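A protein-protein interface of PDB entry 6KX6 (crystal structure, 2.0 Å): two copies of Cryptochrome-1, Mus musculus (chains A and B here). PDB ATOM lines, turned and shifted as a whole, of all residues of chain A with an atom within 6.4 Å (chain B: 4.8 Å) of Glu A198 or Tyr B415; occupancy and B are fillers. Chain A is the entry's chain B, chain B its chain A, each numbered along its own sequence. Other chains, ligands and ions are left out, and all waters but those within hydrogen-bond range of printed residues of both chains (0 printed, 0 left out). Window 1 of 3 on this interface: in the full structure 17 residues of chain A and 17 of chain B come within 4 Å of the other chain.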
ATOM      1  N   PRO A 195      -3.529   1.642 -22.709  1.00  0.00           N
ATOM      2  CA  PRO A 195      -3.718   0.316 -22.124  1.00  0.00           C
ATOM      3  C   PRO A 195      -5.072   0.196 -21.442  1.00  0.00           C
ATOM      4  O   PRO A 195      -5.729   1.186 -21.114  1.00  0.00           O
ATOM      5  CB  PRO A 195      -2.577   0.221 -21.109  1.00  0.00           C
ATOM      6  CG  PRO A 195      -2.396   1.638 -20.656  1.00  0.00           C
ATOM      7  CD  PRO A 195      -2.714   2.516 -21.848  1.00  0.00           C
ATOM      8  N   SER A 196      -5.486  -1.049 -21.246  1.00  0.00           N
ATOM      9  CA  SER A 196      -6.667  -1.341 -20.455  1.00  0.00           C
ATOM     10  C   SER A 196      -6.286  -1.470 -18.982  1.00  0.00           C
ATOM     11  O   SER A 196      -5.108  -1.516 -18.619  1.00  0.00           O
ATOM     12  CB  SER A 196      -7.344  -2.619 -20.949  1.00  0.00           C
ATOM     13  OG  SER A 196      -6.476  -3.732 -20.821  1.00  0.00           O
ATOM     14  N   LEU A 197      -7.311  -1.518 -18.127  1.00  0.00           N
ATOM     15  CA  LEU A 197      -7.075  -1.678 -16.696  1.00  0.00           C
ATOM     16  C   LEU A 197      -6.343  -2.981 -16.400  1.00  0.00           C
ATOM     17  O   LEU A 197      -5.436  -3.014 -15.560  1.00  0.00           O
ATOM     18  CB  LEU A 197      -8.399  -1.633 -15.935  1.00  0.00           C
ATOM     19  CG  LEU A 197      -9.143  -0.300 -15.859  1.00  0.00           C
ATOM     20  CD1 LEU A 197     -10.599  -0.541 -15.490  1.00  0.00           C
ATOM     21  CD2 LEU A 197      -8.479   0.629 -14.855  1.00  0.00           C
ATOM     22  N   GLU A 198      -6.729  -4.067 -17.072  1.00  0.00           N
ATOM     23  CA  GLU A 198      -6.049  -5.340 -16.861  1.00  0.00           C
ATOM     24  C   GLU A 198      -4.600  -5.273 -17.318  1.00  0.00           C
ATOM     25  O   GLU A 198      -3.727  -5.912 -16.718  1.00  0.00           O
ATOM     26  CB  GLU A 198      -6.790  -6.458 -17.594  1.00  0.00           C
ATOM     27  CG  GLU A 198      -8.241  -6.629 -17.170  1.00  0.00           C
ATOM     28  CD  GLU A 198      -9.203  -5.842 -18.041  1.00  0.00           C
ATOM     29  OE1 GLU A 198      -8.745  -4.954 -18.792  1.00  0.00           O
ATOM     30  OE2 GLU A 198     -10.421  -6.110 -17.973  1.00  0.00           O
ATOM     31  N   GLU A 199      -4.320  -4.502 -18.371  1.00  0.00           N
ATOM     32  CA  GLU A 199      -2.943  -4.329 -18.811  1.00  0.00           C
ATOM     33  C   GLU A 199      -2.116  -3.552 -17.797  1.00  0.00           C
ATOM     34  O   GLU A 199      -0.884  -3.651 -17.813  1.00  0.00           O
ATOM     35  CB  GLU A 199      -2.910  -3.652 -20.183  1.00  0.00           C
ATOM     36  CG  GLU A 199      -2.963  -4.659 -21.333  1.00  0.00           C
ATOM     37  CD  GLU A 199      -3.639  -4.127 -22.581  1.00  0.00           C
ATOM     38  OE1 GLU A 199      -4.729  -3.528 -22.464  1.00  0.00           O
ATOM     39  OE2 GLU A 199      -3.083  -4.329 -23.682  1.00  0.00           O
ATOM     40  N   LEU A 200      -2.763  -2.800 -16.908  1.00  0.00           N
ATOM     41  CA  LEU A 200      -2.087  -2.165 -15.786  1.00  0.00           C
ATOM     42  C   LEU A 200      -2.073  -3.037 -14.537  1.00  0.00           C
ATOM     43  O   LEU A 200      -1.572  -2.596 -13.498  1.00  0.00           O
ATOM     44  CB  LEU A 200      -2.741  -0.817 -15.460  1.00  0.00           C
ATOM     45  CG  LEU A 200      -2.819   0.231 -16.571  1.00  0.00           C
ATOM     46  CD1 LEU A 200      -3.319   1.560 -16.016  1.00  0.00           C
ATOM     47  CD2 LEU A 200      -1.469   0.403 -17.241  1.00  0.00           C
ATOM     48  N   GLY A 201      -2.614  -4.252 -14.606  1.00  0.00           N
ATOM     49  CA  GLY A 201      -2.585  -5.147 -13.466  1.00  0.00           C
ATOM     50  C   GLY A 201      -3.730  -4.991 -12.492  1.00  0.00           C
ATOM     51  O   GLY A 201      -3.628  -5.464 -11.355  1.00  0.00           O
ATOM     52  N   PHE A 202      -4.818  -4.346 -12.899  1.00  0.00           N
ATOM     53  CA  PHE A 202      -5.973  -4.165 -12.033  1.00  0.00           C
ATOM     54  C   PHE A 202      -6.900  -5.372 -12.110  1.00  0.00           C
ATOM     55  O   PHE A 202      -7.031  -6.016 -13.154  1.00  0.00           O
ATOM     56  CB  PHE A 202      -6.747  -2.902 -12.417  1.00  0.00           C
ATOM     57  CG  PHE A 202      -6.386  -1.696 -11.597  1.00  0.00           C
ATOM     58  CD1 PHE A 202      -6.775  -1.601 -10.271  1.00  0.00           C
ATOM     59  CD2 PHE A 202      -5.662  -0.656 -12.154  1.00  0.00           C
ATOM     60  CE1 PHE A 202      -6.443  -0.493  -9.515  1.00  0.00           C
ATOM     61  CE2 PHE A 202      -5.328   0.454 -11.404  1.00  0.00           C
ATOM     62  CZ  PHE A 202      -5.720   0.535 -10.082  1.00  0.00           C
ATOM     63  N   ASP A 203      -7.547  -5.673 -10.986  1.00  0.00           N
ATOM     64  CA  ASP A 203      -8.585  -6.698 -10.930  1.00  0.00           C
ATOM     65  C   ASP A 203      -9.911  -6.044 -11.301  1.00  0.00           C
ATOM     66  O   ASP A 203     -10.460  -5.255 -10.524  1.00  0.00           O
ATOM     67  CB  ASP A 203      -8.650  -7.334  -9.543  1.00  0.00           C
ATOM     68  CG  ASP A 203      -9.846  -8.262  -9.378  1.00  0.00           C
ATOM     69  OD1 ASP A 203     -10.239  -8.919 -10.366  1.00  0.00           O
ATOM     70  OD2 ASP A 203     -10.396  -8.335  -8.257  1.00  0.00           O
ATOM     71  N   THR A 204     -10.425  -6.369 -12.487  1.00  0.00           N
ATOM     72  CA  THR A 204     -11.656  -5.783 -13.000  1.00  0.00           C
ATOM     73  C   THR A 204     -12.848  -6.726 -12.897  1.00  0.00           C
ATOM     74  O   THR A 204     -13.910  -6.427 -13.452  1.00  0.00           O
ATOM     75  CB  THR A 204     -11.468  -5.357 -14.459  1.00  0.00           C
ATOM     76  OG1 THR A 204     -10.981  -6.468 -15.224  1.00  0.00           O
ATOM     77  CG2 THR A 204     -10.468  -4.212 -14.552  1.00  0.00           C
ATOM     78  N   LEU B 358      -4.740 -13.235 -14.890  1.00  0.00           N
ATOM     79  CA  LEU B 358      -4.712 -12.280 -15.992  1.00  0.00           C
ATOM     80  C   LEU B 358      -4.132 -12.890 -17.261  1.00  0.00           C
ATOM     81  O   LEU B 358      -4.443 -12.428 -18.366  1.00  0.00           O
ATOM     82  CB  LEU B 358      -3.922 -11.037 -15.585  1.00  0.00           C
ATOM     83  CG  LEU B 358      -4.615 -10.129 -14.568  1.00  0.00           C
ATOM     84  CD1 LEU B 358      -3.752  -8.917 -14.261  1.00  0.00           C
ATOM     85  CD2 LEU B 358      -5.990  -9.704 -15.066  1.00  0.00           C
ATOM     86  N   HIS B 361      -7.135 -14.454 -18.936  1.00  0.00           N
ATOM     87  CA  HIS B 361      -7.815 -13.419 -19.713  1.00  0.00           C
ATOM     88  C   HIS B 361      -7.128 -13.192 -21.055  1.00  0.00           C
ATOM     89  O   HIS B 361      -7.792 -13.077 -22.093  1.00  0.00           O
ATOM     90  CB  HIS B 361      -7.854 -12.105 -18.928  1.00  0.00           C
ATOM     91  CG  HIS B 361      -8.800 -12.106 -17.767  1.00  0.00           C
ATOM     92  ND1 HIS B 361      -9.004 -13.210 -16.967  1.00  0.00           N
ATOM     93  CD2 HIS B 361      -9.590 -11.127 -17.264  1.00  0.00           C
ATOM     94  CE1 HIS B 361      -9.882 -12.913 -16.026  1.00  0.00           C
ATOM     95  NE2 HIS B 361     -10.253 -11.656 -16.184  1.00  0.00           N
ATOM     96  N   ALA B 362      -5.794 -13.118 -21.049  1.00  0.00           N
ATOM     97  CA  ALA B 362      -5.053 -12.793 -22.265  1.00  0.00           C
ATOM     98  C   ALA B 362      -5.272 -13.842 -23.350  1.00  0.00           C
ATOM     99  O   ALA B 362      -5.570 -13.505 -24.502  1.00  0.00           O
ATOM    100  CB  ALA B 362      -3.563 -12.652 -21.946  1.00  0.00           C
ATOM    101  N   CYS B 365      -9.049 -13.983 -24.544  1.00  0.00           N
ATOM    102  CA  CYS B 365      -9.444 -12.910 -25.446  1.00  0.00           C
ATOM    103  C   CYS B 365      -8.841 -13.128 -26.828  1.00  0.00           C
ATOM    104  O   CYS B 365      -9.517 -12.942 -27.844  1.00  0.00           O
ATOM    105  CB  CYS B 365      -9.037 -11.554 -24.861  1.00  0.00           C
ATOM    106  SG  CYS B 365      -9.138 -10.154 -26.006  1.00  0.00           S
ATOM    107  N   ARG B 369     -13.067 -13.339 -28.625  1.00  0.00           N
ATOM    108  CA  ARG B 369     -13.515 -12.020 -29.059  1.00  0.00           C
ATOM    109  C   ARG B 369     -12.390 -11.178 -29.649  1.00  0.00           C
ATOM    110  O   ARG B 369     -12.663 -10.258 -30.428  1.00  0.00           O
ATOM    111  CB  ARG B 369     -14.156 -11.272 -27.886  1.00  0.00           C
ATOM    112  CG  ARG B 369     -13.212 -11.065 -26.709  1.00  0.00           C
ATOM    113  CD  ARG B 369     -13.815 -10.185 -25.616  1.00  0.00           C
ATOM    114  NE  ARG B 369     -12.828  -9.253 -25.067  1.00  0.00           N
ATOM    115  CZ  ARG B 369     -12.189  -9.425 -23.912  1.00  0.00           C
ATOM    116  NH1 ARG B 369     -11.307  -8.525 -23.496  1.00  0.00           N
ATOM    117  NH2 ARG B 369     -12.431 -10.495 -23.168  1.00  0.00           N
ATOM    118  N   CYS B 414     -10.110  -5.087 -25.990  1.00  0.00           N
ATOM    119  CA  CYS B 414      -9.228  -6.105 -26.553  1.00  0.00           C
ATOM    120  C   CYS B 414      -7.787  -5.937 -26.071  1.00  0.00           C
ATOM    121  O   CYS B 414      -7.152  -4.916 -26.330  1.00  0.00           O
ATOM    122  CB  CYS B 414      -9.275  -6.062 -28.082  1.00  0.00           C
ATOM    123  SG  CYS B 414      -8.440  -7.438 -28.907  1.00  0.00           S
ATOM    124  N   TYR B 415      -7.279  -6.950 -25.372  1.00  0.00           N
ATOM    125  CA  TYR B 415      -5.897  -6.925 -24.916  1.00  0.00           C
ATOM    126  C   TYR B 415      -4.942  -6.992 -26.103  1.00  0.00           C
ATOM    127  O   TYR B 415      -5.232  -7.613 -27.129  1.00  0.00           O
ATOM    128  CB  TYR B 415      -5.625  -8.099 -23.973  1.00  0.00           C
ATOM    129  CG  TYR B 415      -6.585  -8.213 -22.812  1.00  0.00           C
ATOM    130  CD1 TYR B 415      -6.805  -7.145 -21.952  1.00  0.00           C
ATOM    131  CD2 TYR B 415      -7.271  -9.395 -22.573  1.00  0.00           C
ATOM    132  CE1 TYR B 415      -7.684  -7.257 -20.888  1.00  0.00           C
ATOM    133  CE2 TYR B 415      -8.149  -9.515 -21.514  1.00  0.00           C
ATOM    134  CZ  TYR B 415      -8.351  -8.446 -20.674  1.00  0.00           C
ATOM    135  OH  TYR B 415      -9.226  -8.567 -19.620  1.00  0.00           O
ATOM    136  N   CYS B 416      -3.789  -6.339 -25.961  1.00  0.00           N
ATOM    137  CA  CYS B 416      -2.819  -6.448 -27.044  1.00  0.00           C
ATOM    138  C   CYS B 416      -1.885  -7.622 -26.777  1.00  0.00           C
ATOM    139  O   CYS B 416      -1.293  -7.697 -25.698  1.00  0.00           O
ATOM    140  CB  CYS B 416      -2.010  -5.166 -27.180  1.00  0.00           C
ATOM    141  SG  CYS B 416      -0.715  -5.199 -28.437  1.00  0.00           S
ATOM    142  N   PRO B 417      -1.739  -8.558 -27.722  1.00  0.00           N
ATOM    143  CA  PRO B 417      -0.876  -9.726 -27.480  1.00  0.00           C
ATOM    144  C   PRO B 417       0.608  -9.401 -27.495  1.00  0.00           C
ATOM    145  O   PRO B 417       1.419 -10.292 -27.209  1.00  0.00           O
ATOM    146  CB  PRO B 417      -1.253 -10.677 -28.620  1.00  0.00           C
ATOM    147  CG  PRO B 417      -1.678  -9.773 -29.724  1.00  0.00           C
ATOM    148  CD  PRO B 417      -2.384  -8.620 -29.045  1.00  0.00           C
ATOM    149  N   PHE B 420       0.527  -6.253 -23.710  1.00  0.00           N
ATOM    150  CA  PHE B 420       0.191  -6.731 -22.370  1.00  0.00           C
ATOM    151  C   PHE B 420       1.389  -7.408 -21.714  1.00  0.00           C
ATOM    152  O   PHE B 420       1.728  -7.117 -20.561  1.00  0.00           O
ATOM    153  CB  PHE B 420      -1.011  -7.679 -22.422  1.00  0.00           C
ATOM    154  CG  PHE B 420      -1.651  -7.938 -21.073  1.00  0.00           C
ATOM    155  CD1 PHE B 420      -1.197  -7.291 -19.931  1.00  0.00           C
ATOM    156  CD2 PHE B 420      -2.709  -8.820 -20.950  1.00  0.00           C
ATOM    157  CE1 PHE B 420      -1.775  -7.530 -18.697  1.00  0.00           C
ATOM    158  CE2 PHE B 420      -3.299  -9.056 -19.714  1.00  0.00           C
ATOM    159  CZ  PHE B 420      -2.828  -8.407 -18.589  1.00  0.00           C
ATOM    160  N   HIS B 475      -2.692  -8.445 -35.595  1.00  0.00           N
ATOM    161  CA  HIS B 475      -3.548  -8.169 -34.442  1.00  0.00           C
ATOM    162  C   HIS B 475      -4.397  -6.926 -34.661  1.00  0.00           C
ATOM    163  O   HIS B 475      -5.598  -6.923 -34.365  1.00  0.00           O
ATOM    164  CB  HIS B 475      -2.723  -7.999 -33.170  1.00  0.00           C
ATOM    165  CG  HIS B 475      -3.511  -7.421 -32.035  1.00  0.00           C
ATOM    166  ND1 HIS B 475      -4.554  -8.098 -31.438  1.00  0.00           N
ATOM    167  CD2 HIS B 475      -3.439  -6.219 -31.415  1.00  0.00           C
ATOM    168  CE1 HIS B 475      -5.078  -7.346 -30.488  1.00  0.00           C
ATOM    169  NE2 HIS B 475      -4.418  -6.201 -30.450  1.00  0.00           N
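Ser A196 touches Tyr B415. Glu A198 touches Leu B358 (O to CD1, 3.9 Å). Glu A198 touches Phe B420 (O to CE1, 3.2 Å). Glu A199 touches Phe B420.
The side-chain carboxylate (OE2) of Glu A199 lies within hydrogen-bond range of the backbone NH (N) of Cys B416, at 3.1 Å. The side-chain hydroxyl (OH) of Tyr B415 sits close to the side-chain carboxylate (OE2) of Glu A198 (3.2 Å).
OE1 of Glu A199 is in hydrogen-bond range of OG of Ser A196, 2.4 Å away. N of Tyr B415 lies within hydrogen-bond range of SG of Cys B365 (3.8 Å). OG of Ser A196 is in hydrogen-bond range of OE1 of Glu A198, 3.3 Å away. The side-chain carboxylate (OE2) of Glu A198 sits at hydrogen-bond distance from the side-chain hydroxyl (OG1) of Thr A204, at 2.8 Å.
Of the printed residues of chain B, Ser A196 touches Tyr B415 (3.6 Å). Leu A197 touches none of the printed residues of chain B. Glu A198 touches just these residues of chain B: Leu B358 (3.9 Å), Tyr B415 (3.1 Å) and Phe B420 (3.2 Å). Gly A201 touches none of the printed residues of chain B. Of the printed residues of chain A, Leu B358 touches Glu A198 (3.9 Å). Of chain A, only Ser A196 and Glu A198 come within 4 Å of Tyr B415. The nearest printed residue of chain A that does not touch Cys B416 is Ser A196 (6.4 Å).
No position is printed for both chains. Of the 6 pairs that touch across the chains among the printed residues, none has its exchanged pair printed and touching as well.
Hydrophobic or aromatic side chains of chain B within 4 Å of the printed part of chain A: Leu B358, Tyr B415 and Phe B420. Among the printed residues, 6 pairs touch across the chains. Among the printed residues, no Asp or Glu carboxylate lies within 4 Å of a Lys or Arg side-chain nitrogen of the other chain.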
